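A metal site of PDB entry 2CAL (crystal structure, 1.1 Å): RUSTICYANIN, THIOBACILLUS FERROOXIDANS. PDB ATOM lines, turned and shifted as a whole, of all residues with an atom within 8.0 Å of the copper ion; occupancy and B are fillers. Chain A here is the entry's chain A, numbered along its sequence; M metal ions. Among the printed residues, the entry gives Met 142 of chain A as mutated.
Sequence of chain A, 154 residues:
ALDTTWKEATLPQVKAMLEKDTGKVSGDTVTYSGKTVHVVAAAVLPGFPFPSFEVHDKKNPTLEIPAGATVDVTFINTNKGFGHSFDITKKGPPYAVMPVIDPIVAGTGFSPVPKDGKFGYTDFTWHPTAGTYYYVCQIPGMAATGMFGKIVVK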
ATOM      1  N   ALA A  43     -18.010 -25.843 -26.598  1.00  0.00           N
ATOM      2  CA  ALA A  43     -18.818 -25.713 -25.382  1.00  0.00           C
ATOM      3  C   ALA A  43     -18.657 -24.308 -24.759  1.00  0.00           C
ATOM      4  O   ALA A  43     -17.557 -24.016 -24.249  1.00  0.00           O
ATOM      5  CB  ALA A  43     -18.398 -26.778 -24.383  1.00  0.00           C
ATOM      6  N   VAL A  44     -19.684 -23.506 -24.827  1.00  0.00           N
ATOM      7  CA  VAL A  44     -19.820 -22.187 -24.214  1.00  0.00           C
ATOM      8  C   VAL A  44     -18.604 -21.298 -24.615  1.00  0.00           C
ATOM      9  O   VAL A  44     -17.661 -21.027 -23.868  1.00  0.00           O
ATOM     10  CB  VAL A  44     -19.975 -22.180 -22.675  1.00  0.00           C
ATOM     11  CG1 VAL A  44     -20.442 -20.826 -22.180  1.00  0.00           C
ATOM     12  CG2 VAL A  44     -20.960 -23.253 -22.216  1.00  0.00           C
ATOM     13  N   PHE A  50     -24.786 -19.753 -21.082  1.00  0.00           N
ATOM     14  CA  PHE A  50     -24.467 -20.971 -20.372  1.00  0.00           C
ATOM     15  C   PHE A  50     -25.754 -21.730 -20.006  1.00  0.00           C
ATOM     16  O   PHE A  50     -26.639 -21.119 -19.406  1.00  0.00           O
ATOM     17  CB  PHE A  50     -23.710 -20.751 -19.038  1.00  0.00           C
ATOM     18  CG  PHE A  50     -23.332 -21.986 -18.231  1.00  0.00           C
ATOM     19  CD1 PHE A  50     -24.194 -22.456 -17.232  1.00  0.00           C
ATOM     20  CD2 PHE A  50     -22.163 -22.743 -18.335  1.00  0.00           C
ATOM     21  CE1 PHE A  50     -23.980 -23.559 -16.458  1.00  0.00           C
ATOM     22  CE2 PHE A  50     -21.947 -23.895 -17.573  1.00  0.00           C
ATOM     23  CZ  PHE A  50     -22.825 -24.317 -16.634  1.00  0.00           C
ATOM     24  N   PRO A  51     -25.823 -23.049 -20.170  1.00  0.00           N
ATOM     25  CA  PRO A  51     -24.933 -23.929 -20.906  1.00  0.00           C
ATOM     26  C   PRO A  51     -25.401 -24.136 -22.336  1.00  0.00           C
ATOM     27  O   PRO A  51     -26.570 -24.357 -22.626  1.00  0.00           O
ATOM     28  CB  PRO A  51     -25.027 -25.246 -20.103  1.00  0.00           C
ATOM     29  CG  PRO A  51     -26.480 -25.280 -19.716  1.00  0.00           C
ATOM     30  CD  PRO A  51     -26.892 -23.859 -19.504  1.00  0.00           C
ATOM     31  N   SER A  52     -24.467 -24.123 -23.285  1.00  0.00           N
ATOM     32  CA  SER A  52     -24.812 -24.258 -24.708  1.00  0.00           C
ATOM     33  C   SER A  52     -23.606 -24.694 -25.489  1.00  0.00           C
ATOM     34  O   SER A  52     -22.438 -24.577 -25.067  1.00  0.00           O
ATOM     35  CB  SER A  52     -25.352 -22.959 -25.297  1.00  0.00           C
ATOM     36  OG  SER A  52     -24.296 -21.967 -25.393  1.00  0.00           O
ATOM     37  N   PHE A  53     -23.857 -25.232 -26.684  1.00  0.00           N
ATOM     38  CA  PHE A  53     -22.865 -25.460 -27.722  1.00  0.00           C
ATOM     39  C   PHE A  53     -22.960 -24.355 -28.795  1.00  0.00           C
ATOM     40  O   PHE A  53     -24.097 -23.970 -29.130  1.00  0.00           O
ATOM     41  CB  PHE A  53     -23.105 -26.794 -28.443  1.00  0.00           C
ATOM     42  CG  PHE A  53     -22.974 -28.040 -27.587  1.00  0.00           C
ATOM     43  CD1 PHE A  53     -21.716 -28.527 -27.248  1.00  0.00           C
ATOM     44  CD2 PHE A  53     -24.103 -28.720 -27.145  1.00  0.00           C
ATOM     45  CE1 PHE A  53     -21.604 -29.722 -26.531  1.00  0.00           C
ATOM     46  CE2 PHE A  53     -24.005 -29.916 -26.454  1.00  0.00           C
ATOM     47  CZ  PHE A  53     -22.749 -30.408 -26.153  1.00  0.00           C
ATOM     48  N   PHE A  75     -14.472 -31.060 -31.561  1.00  0.00           N
ATOM     49  CA  PHE A  75     -15.123 -30.518 -30.373  1.00  0.00           C
ATOM     50  C   PHE A  75     -14.083 -29.895 -29.438  1.00  0.00           C
ATOM     51  O   PHE A  75     -13.091 -30.551 -29.117  1.00  0.00           O
ATOM     52  CB  PHE A  75     -15.896 -31.633 -29.635  1.00  0.00           C
ATOM     53  CG  PHE A  75     -16.477 -31.160 -28.305  1.00  0.00           C
ATOM     54  CD1 PHE A  75     -17.362 -30.102 -28.207  1.00  0.00           C
ATOM     55  CD2 PHE A  75     -16.088 -31.800 -27.136  1.00  0.00           C
ATOM     56  CE1 PHE A  75     -17.874 -29.675 -27.007  1.00  0.00           C
ATOM     57  CE2 PHE A  75     -16.608 -31.390 -25.900  1.00  0.00           C
ATOM     58  CZ  PHE A  75     -17.465 -30.324 -25.837  1.00  0.00           C
ATOM     59  N   ASN A  77     -13.566 -27.601 -25.846  1.00  0.00           N
ATOM     60  CA  ASN A  77     -14.167 -27.099 -24.609  1.00  0.00           C
ATOM     61  C   ASN A  77     -13.513 -25.797 -24.179  1.00  0.00           C
ATOM     62  O   ASN A  77     -12.394 -25.822 -23.644  1.00  0.00           O
ATOM     63  CB  ASN A  77     -14.053 -28.118 -23.480  1.00  0.00           C
ATOM     64  CG  ASN A  77     -14.598 -27.642 -22.174  1.00  0.00           C
ATOM     65  OD1 ASN A  77     -14.182 -28.141 -21.068  1.00  0.00           O
ATOM     66  ND2 ASN A  77     -15.470 -26.677 -22.185  1.00  0.00           N
ATOM     67  N   ASN A  79     -15.028 -23.695 -21.905  1.00  0.00           N
ATOM     68  CA  ASN A  79     -15.724 -23.196 -20.703  1.00  0.00           C
ATOM     69  C   ASN A  79     -14.950 -23.493 -19.439  1.00  0.00           C
ATOM     70  O   ASN A  79     -14.836 -24.620 -18.994  1.00  0.00           O
ATOM     71  CB  ASN A  79     -17.117 -23.824 -20.672  1.00  0.00           C
ATOM     72  CG  ASN A  79     -18.042 -23.161 -19.707  1.00  0.00           C
ATOM     73  OD1 ASN A  79     -17.951 -21.967 -19.337  1.00  0.00           O
ATOM     74  ND2 ASN A  79     -18.952 -23.920 -19.195  1.00  0.00           N
ATOM     75  N   PHE A  82     -15.327 -26.355 -16.345  1.00  0.00           N
ATOM     76  CA  PHE A  82     -16.238 -27.444 -16.712  1.00  0.00           C
ATOM     77  C   PHE A  82     -15.558 -28.453 -17.616  1.00  0.00           C
ATOM     78  O   PHE A  82     -14.567 -28.107 -18.293  1.00  0.00           O
ATOM     79  CB  PHE A  82     -17.487 -26.887 -17.400  1.00  0.00           C
ATOM     80  CG  PHE A  82     -18.345 -26.069 -16.448  1.00  0.00           C
ATOM     81  CD1 PHE A  82     -18.042 -24.762 -16.189  1.00  0.00           C
ATOM     82  CD2 PHE A  82     -19.391 -26.661 -15.821  1.00  0.00           C
ATOM     83  CE1 PHE A  82     -18.803 -24.025 -15.308  1.00  0.00           C
ATOM     84  CE2 PHE A  82     -20.205 -25.963 -14.937  1.00  0.00           C
ATOM     85  CZ  PHE A  82     -19.870 -24.653 -14.681  1.00  0.00           C
ATOM     86  N   GLY A  83     -16.105 -29.671 -17.653  1.00  0.00           N
ATOM     87  CA  GLY A  83     -15.595 -30.745 -18.493  1.00  0.00           C
ATOM     88  C   GLY A  83     -16.624 -31.325 -19.473  1.00  0.00           C
ATOM     89  O   GLY A  83     -16.784 -32.542 -19.588  1.00  0.00           O
ATOM     90  N   HIS A  84     -17.277 -30.466 -20.228  1.00  0.00           N
ATOM     91  CA  HIS A  84     -18.383 -30.795 -21.120  1.00  0.00           C
ATOM     92  C   HIS A  84     -18.008 -31.919 -22.093  1.00  0.00           C
ATOM     93  O   HIS A  84     -16.820 -32.054 -22.498  1.00  0.00           O
ATOM     94  CB  HIS A  84     -18.767 -29.550 -21.901  1.00  0.00           C
ATOM     95  CG  HIS A  84     -19.189 -28.371 -21.081  1.00  0.00           C
ATOM     96  ND1 HIS A  84     -20.438 -28.257 -20.497  1.00  0.00           N
ATOM     97  CD2 HIS A  84     -18.535 -27.235 -20.843  1.00  0.00           C
ATOM     98  CE1 HIS A  84     -20.413 -27.051 -19.922  1.00  0.00           C
ATOM     99  NE2 HIS A  84     -19.314 -26.433 -20.060  1.00  0.00           N
ATOM    100  N   SER A  85     -19.018 -32.661 -22.445  1.00  0.00           N
ATOM    101  CA  SER A  85     -18.892 -33.687 -23.487  1.00  0.00           C
ATOM    102  C   SER A  85     -19.739 -33.301 -24.693  1.00  0.00           C
ATOM    103  O   SER A  85     -20.612 -32.441 -24.617  1.00  0.00           O
ATOM    104  CB  SER A  85     -19.325 -35.075 -22.956  1.00  0.00           C
ATOM    105  OG  SER A  85     -20.705 -35.139 -22.758  1.00  0.00           O
ATOM    106  N   PHE A  86     -19.523 -34.031 -25.789  1.00  0.00           N
ATOM    107  CA  PHE A  86     -20.273 -33.895 -27.033  1.00  0.00           C
ATOM    108  C   PHE A  86     -20.624 -35.308 -27.455  1.00  0.00           C
ATOM    109  O   PHE A  86     -19.787 -36.020 -27.989  1.00  0.00           O
ATOM    110  CB  PHE A  86     -19.472 -33.113 -28.103  1.00  0.00           C
ATOM    111  CG  PHE A  86     -20.242 -32.830 -29.384  1.00  0.00           C
ATOM    112  CD1 PHE A  86     -20.756 -31.557 -29.594  1.00  0.00           C
ATOM    113  CD2 PHE A  86     -20.424 -33.806 -30.374  1.00  0.00           C
ATOM    114  CE1 PHE A  86     -21.437 -31.282 -30.767  1.00  0.00           C
ATOM    115  CE2 PHE A  86     -21.093 -33.537 -31.558  1.00  0.00           C
ATOM    116  CZ  PHE A  86     -21.596 -32.249 -31.725  1.00  0.00           C
ATOM    117  N   PHE A 110     -15.812 -37.016 -21.244  1.00  0.00           N
ATOM    118  CA  PHE A 110     -15.728 -35.703 -20.650  1.00  0.00           C
ATOM    119  C   PHE A 110     -14.379 -35.077 -21.076  1.00  0.00           C
ATOM    120  O   PHE A 110     -13.327 -35.689 -21.060  1.00  0.00           O
ATOM    121  CB  PHE A 110     -15.841 -35.796 -19.126  1.00  0.00           C
ATOM    122  CG  PHE A 110     -17.236 -36.257 -18.757  1.00  0.00           C
ATOM    123  CD1 PHE A 110     -18.361 -35.557 -19.032  1.00  0.00           C
ATOM    124  CD2 PHE A 110     -17.404 -37.497 -18.116  1.00  0.00           C
ATOM    125  CE1 PHE A 110     -19.645 -35.974 -18.740  1.00  0.00           C
ATOM    126  CE2 PHE A 110     -18.681 -37.918 -17.814  1.00  0.00           C
ATOM    127  CZ  PHE A 110     -19.815 -37.195 -18.091  1.00  0.00           C
ATOM    128  N   SER A 111     -14.459 -33.801 -21.431  1.00  0.00           N
ATOM    129  CA  SER A 111     -13.247 -33.100 -21.877  1.00  0.00           C
ATOM    130  C   SER A 111     -12.384 -32.637 -20.719  1.00  0.00           C
ATOM    131  O   SER A 111     -12.891 -32.383 -19.599  1.00  0.00           O
ATOM    132  CB  SER A 111     -13.667 -31.868 -22.683  1.00  0.00           C
ATOM    133  OG  SER A 111     -14.446 -30.951 -21.937  1.00  0.00           O
ATOM    134  N   VAL A 136     -25.565 -33.837 -27.351  1.00  0.00           N
ATOM    135  CA  VAL A 136     -25.917 -33.623 -25.965  1.00  0.00           C
ATOM    136  C   VAL A 136     -24.656 -33.639 -25.109  1.00  0.00           C
ATOM    137  O   VAL A 136     -23.734 -34.433 -25.300  1.00  0.00           O
ATOM    138  CB  VAL A 136     -26.880 -34.742 -25.522  1.00  0.00           C
ATOM    139  CG1 VAL A 136     -27.436 -34.594 -24.102  1.00  0.00           C
ATOM    140  CG2 VAL A 136     -28.086 -34.917 -26.455  1.00  0.00           C
ATOM    141  N   CYS A 137     -24.651 -32.787 -24.072  1.00  0.00           N
ATOM    142  CA  CYS A 137     -23.663 -32.853 -23.011  1.00  0.00           C
ATOM    143  C   CYS A 137     -24.147 -33.758 -21.856  1.00  0.00           C
ATOM    144  O   CYS A 137     -25.311 -33.669 -21.467  1.00  0.00           O
ATOM    145  CB  CYS A 137     -23.357 -31.436 -22.484  1.00  0.00           C
ATOM    146  SG  CYS A 137     -22.101 -31.501 -21.155  1.00  0.00           S
ATOM    147  N   GLN A 138     -23.223 -34.586 -21.384  1.00  0.00           N
ATOM    148  CA  GLN A 138     -23.588 -35.522 -20.307  1.00  0.00           C
ATOM    149  C   GLN A 138     -23.222 -35.036 -18.905  1.00  0.00           C
ATOM    150  O   GLN A 138     -23.484 -35.745 -17.945  1.00  0.00           O
ATOM    151  CB  GLN A 138     -22.845 -36.858 -20.525  1.00  0.00           C
ATOM    152  CG  GLN A 138     -23.469 -37.676 -21.680  1.00  0.00           C
ATOM    153  CD  GLN A 138     -22.962 -39.097 -21.632  1.00  0.00           C
ATOM    154  OE1 GLN A 138     -21.851 -39.541 -21.952  1.00  0.00           O
ATOM    155  NE2 GLN A 138     -23.891 -39.944 -21.223  1.00  0.00           N
ATOM    156  N   ILE A 139     -22.608 -33.861 -18.759  1.00  0.00           N
ATOM    157  CA  ILE A 139     -22.351 -33.367 -17.369  1.00  0.00           C
ATOM    158  C   ILE A 139     -23.682 -33.203 -16.690  1.00  0.00           C
ATOM    159  O   ILE A 139     -24.568 -32.562 -17.252  1.00  0.00           O
ATOM    160  CB  ILE A 139     -21.549 -32.059 -17.409  1.00  0.00           C
ATOM    161  CG1 ILE A 139     -20.124 -32.238 -17.915  1.00  0.00           C
ATOM    162  CG2 ILE A 139     -21.598 -31.428 -16.015  1.00  0.00           C
ATOM    163  CD1 ILE A 139     -19.160 -32.911 -16.976  1.00  0.00           C
ATOM    164  N   PRO A 140     -23.898 -33.741 -15.468  1.00  0.00           N
ATOM    165  CA  PRO A 140     -25.210 -33.633 -14.834  1.00  0.00           C
ATOM    166  C   PRO A 140     -25.794 -32.248 -14.815  1.00  0.00           C
ATOM    167  O   PRO A 140     -25.103 -31.271 -14.485  1.00  0.00           O
ATOM    168  CB  PRO A 140     -24.929 -34.154 -13.408  1.00  0.00           C
ATOM    169  CG  PRO A 140     -23.867 -35.200 -13.696  1.00  0.00           C
ATOM    170  CD  PRO A 140     -22.920 -34.526 -14.692  1.00  0.00           C
ATOM    171  N   GLY A 141     -27.046 -32.145 -15.255  1.00  0.00           N
ATOM    172  CA  GLY A 141     -27.866 -30.962 -15.297  1.00  0.00           C
ATOM    173  C   GLY A 141     -27.780 -30.122 -16.554  1.00  0.00           C
ATOM    174  O   GLY A 141     -28.631 -29.275 -16.762  1.00  0.00           O
ATOM    175  N   MET A 142     -26.728 -30.328 -17.363  1.00  0.00           N
ATOM    176  CA  MET A 142     -26.540 -29.424 -18.475  1.00  0.00           C
ATOM    177  C   MET A 142     -27.557 -29.592 -19.609  1.00  0.00           C
ATOM    178  O   MET A 142     -28.139 -28.633 -20.086  1.00  0.00           O
ATOM    179  CB  MET A 142     -25.143 -29.599 -19.042  1.00  0.00           C
ATOM    180  CG  MET A 142     -24.011 -29.233 -18.082  1.00  0.00           C
ATOM    181  SD  MET A 142     -23.924 -27.525 -17.560  1.00  0.00           S
ATOM    182  CE  MET A 142     -24.757 -27.540 -15.977  1.00  0.00           C
ATOM    183  N   ALA A 143     -27.784 -30.855 -20.022  1.00  0.00           N
ATOM    184  CA  ALA A 143     -28.815 -31.092 -21.055  1.00  0.00           C
ATOM    185  C   ALA A 143     -30.189 -30.700 -20.573  1.00  0.00           C
ATOM    186  O   ALA A 143     -30.976 -30.192 -21.356  1.00  0.00           O
ATOM    187  CB  ALA A 143     -28.728 -32.551 -21.464  1.00  0.00           C
ATOM    188  N   MET A 147     -28.367 -27.662 -22.836  1.00  0.00           N
ATOM    189  CA  MET A 147     -27.129 -27.901 -23.561  1.00  0.00           C
ATOM    190  C   MET A 147     -27.216 -29.115 -24.494  1.00  0.00           C
ATOM    191  O   MET A 147     -26.761 -30.238 -24.238  1.00  0.00           O
ATOM    192  CB  MET A 147     -25.942 -28.051 -22.616  1.00  0.00           C
ATOM    193  CG  MET A 147     -24.615 -27.961 -23.346  1.00  0.00           C
ATOM    194  SD  MET A 147     -23.193 -27.804 -22.235  1.00  0.00           S
ATOM    195  CE  MET A 147     -21.835 -27.621 -23.456  1.00  0.00           C
ATOM    196  N   PHE A 148     -27.909 -28.852 -25.619  1.00  0.00           N
ATOM    197  CA  PHE A 148     -28.144 -29.869 -26.652  1.00  0.00           C
ATOM    198  C   PHE A 148     -28.604 -29.163 -27.909  1.00  0.00           C
ATOM    199  O   PHE A 148     -29.165 -28.056 -27.835  1.00  0.00           O
ATOM    200  CB  PHE A 148     -29.197 -30.949 -26.213  1.00  0.00           C
ATOM    201  CG  PHE A 148     -30.602 -30.423 -26.081  1.00  0.00           C
ATOM    202  CD1 PHE A 148     -31.032 -29.926 -24.828  1.00  0.00           C
ATOM    203  CD2 PHE A 148     -31.513 -30.381 -27.125  1.00  0.00           C
ATOM    204  CE1 PHE A 148     -32.305 -29.434 -24.694  1.00  0.00           C
ATOM    205  CE2 PHE A 148     -32.799 -29.907 -26.978  1.00  0.00           C
ATOM    206  CZ  PHE A 148     -33.180 -29.411 -25.760  1.00  0.00           C
HETATM  207 CU    CU M   1     -21.911 -29.397 -20.784  1.00  0.00          CU
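A ring nitrogen (NE2) of His 84 is in hydrogen-bond range of the side-chain amide nitrogen (ND2) of Asn 79, 2.7 Å away.
The backbone carbonyl oxygen of His 84 sits at hydrogen-bond distance from the side-chain hydroxyl of Ser 111.
The side-chain sulfur (SG) of Cys 137 sits close to the backbone NH (N) of Ile 139.
N of Ser 85 sits close to SG of Cys 137, 3.5 Å away.
O of Met 142 is in hydrogen-bond range of N of Met 147, at 2.9 Å.
Merely in contact with the copper ion: Met 142.
Within 4 Å of the copper ion: His 84, Cys 137, Met 142 and Met 147.
The copper ion is bound by ND1 of His 84.
SG of Cys 137 binds the copper ion (2.1 Å).
The copper ion is bound by SD of Met 147.
The copper ion has three donor atoms within binding distance.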
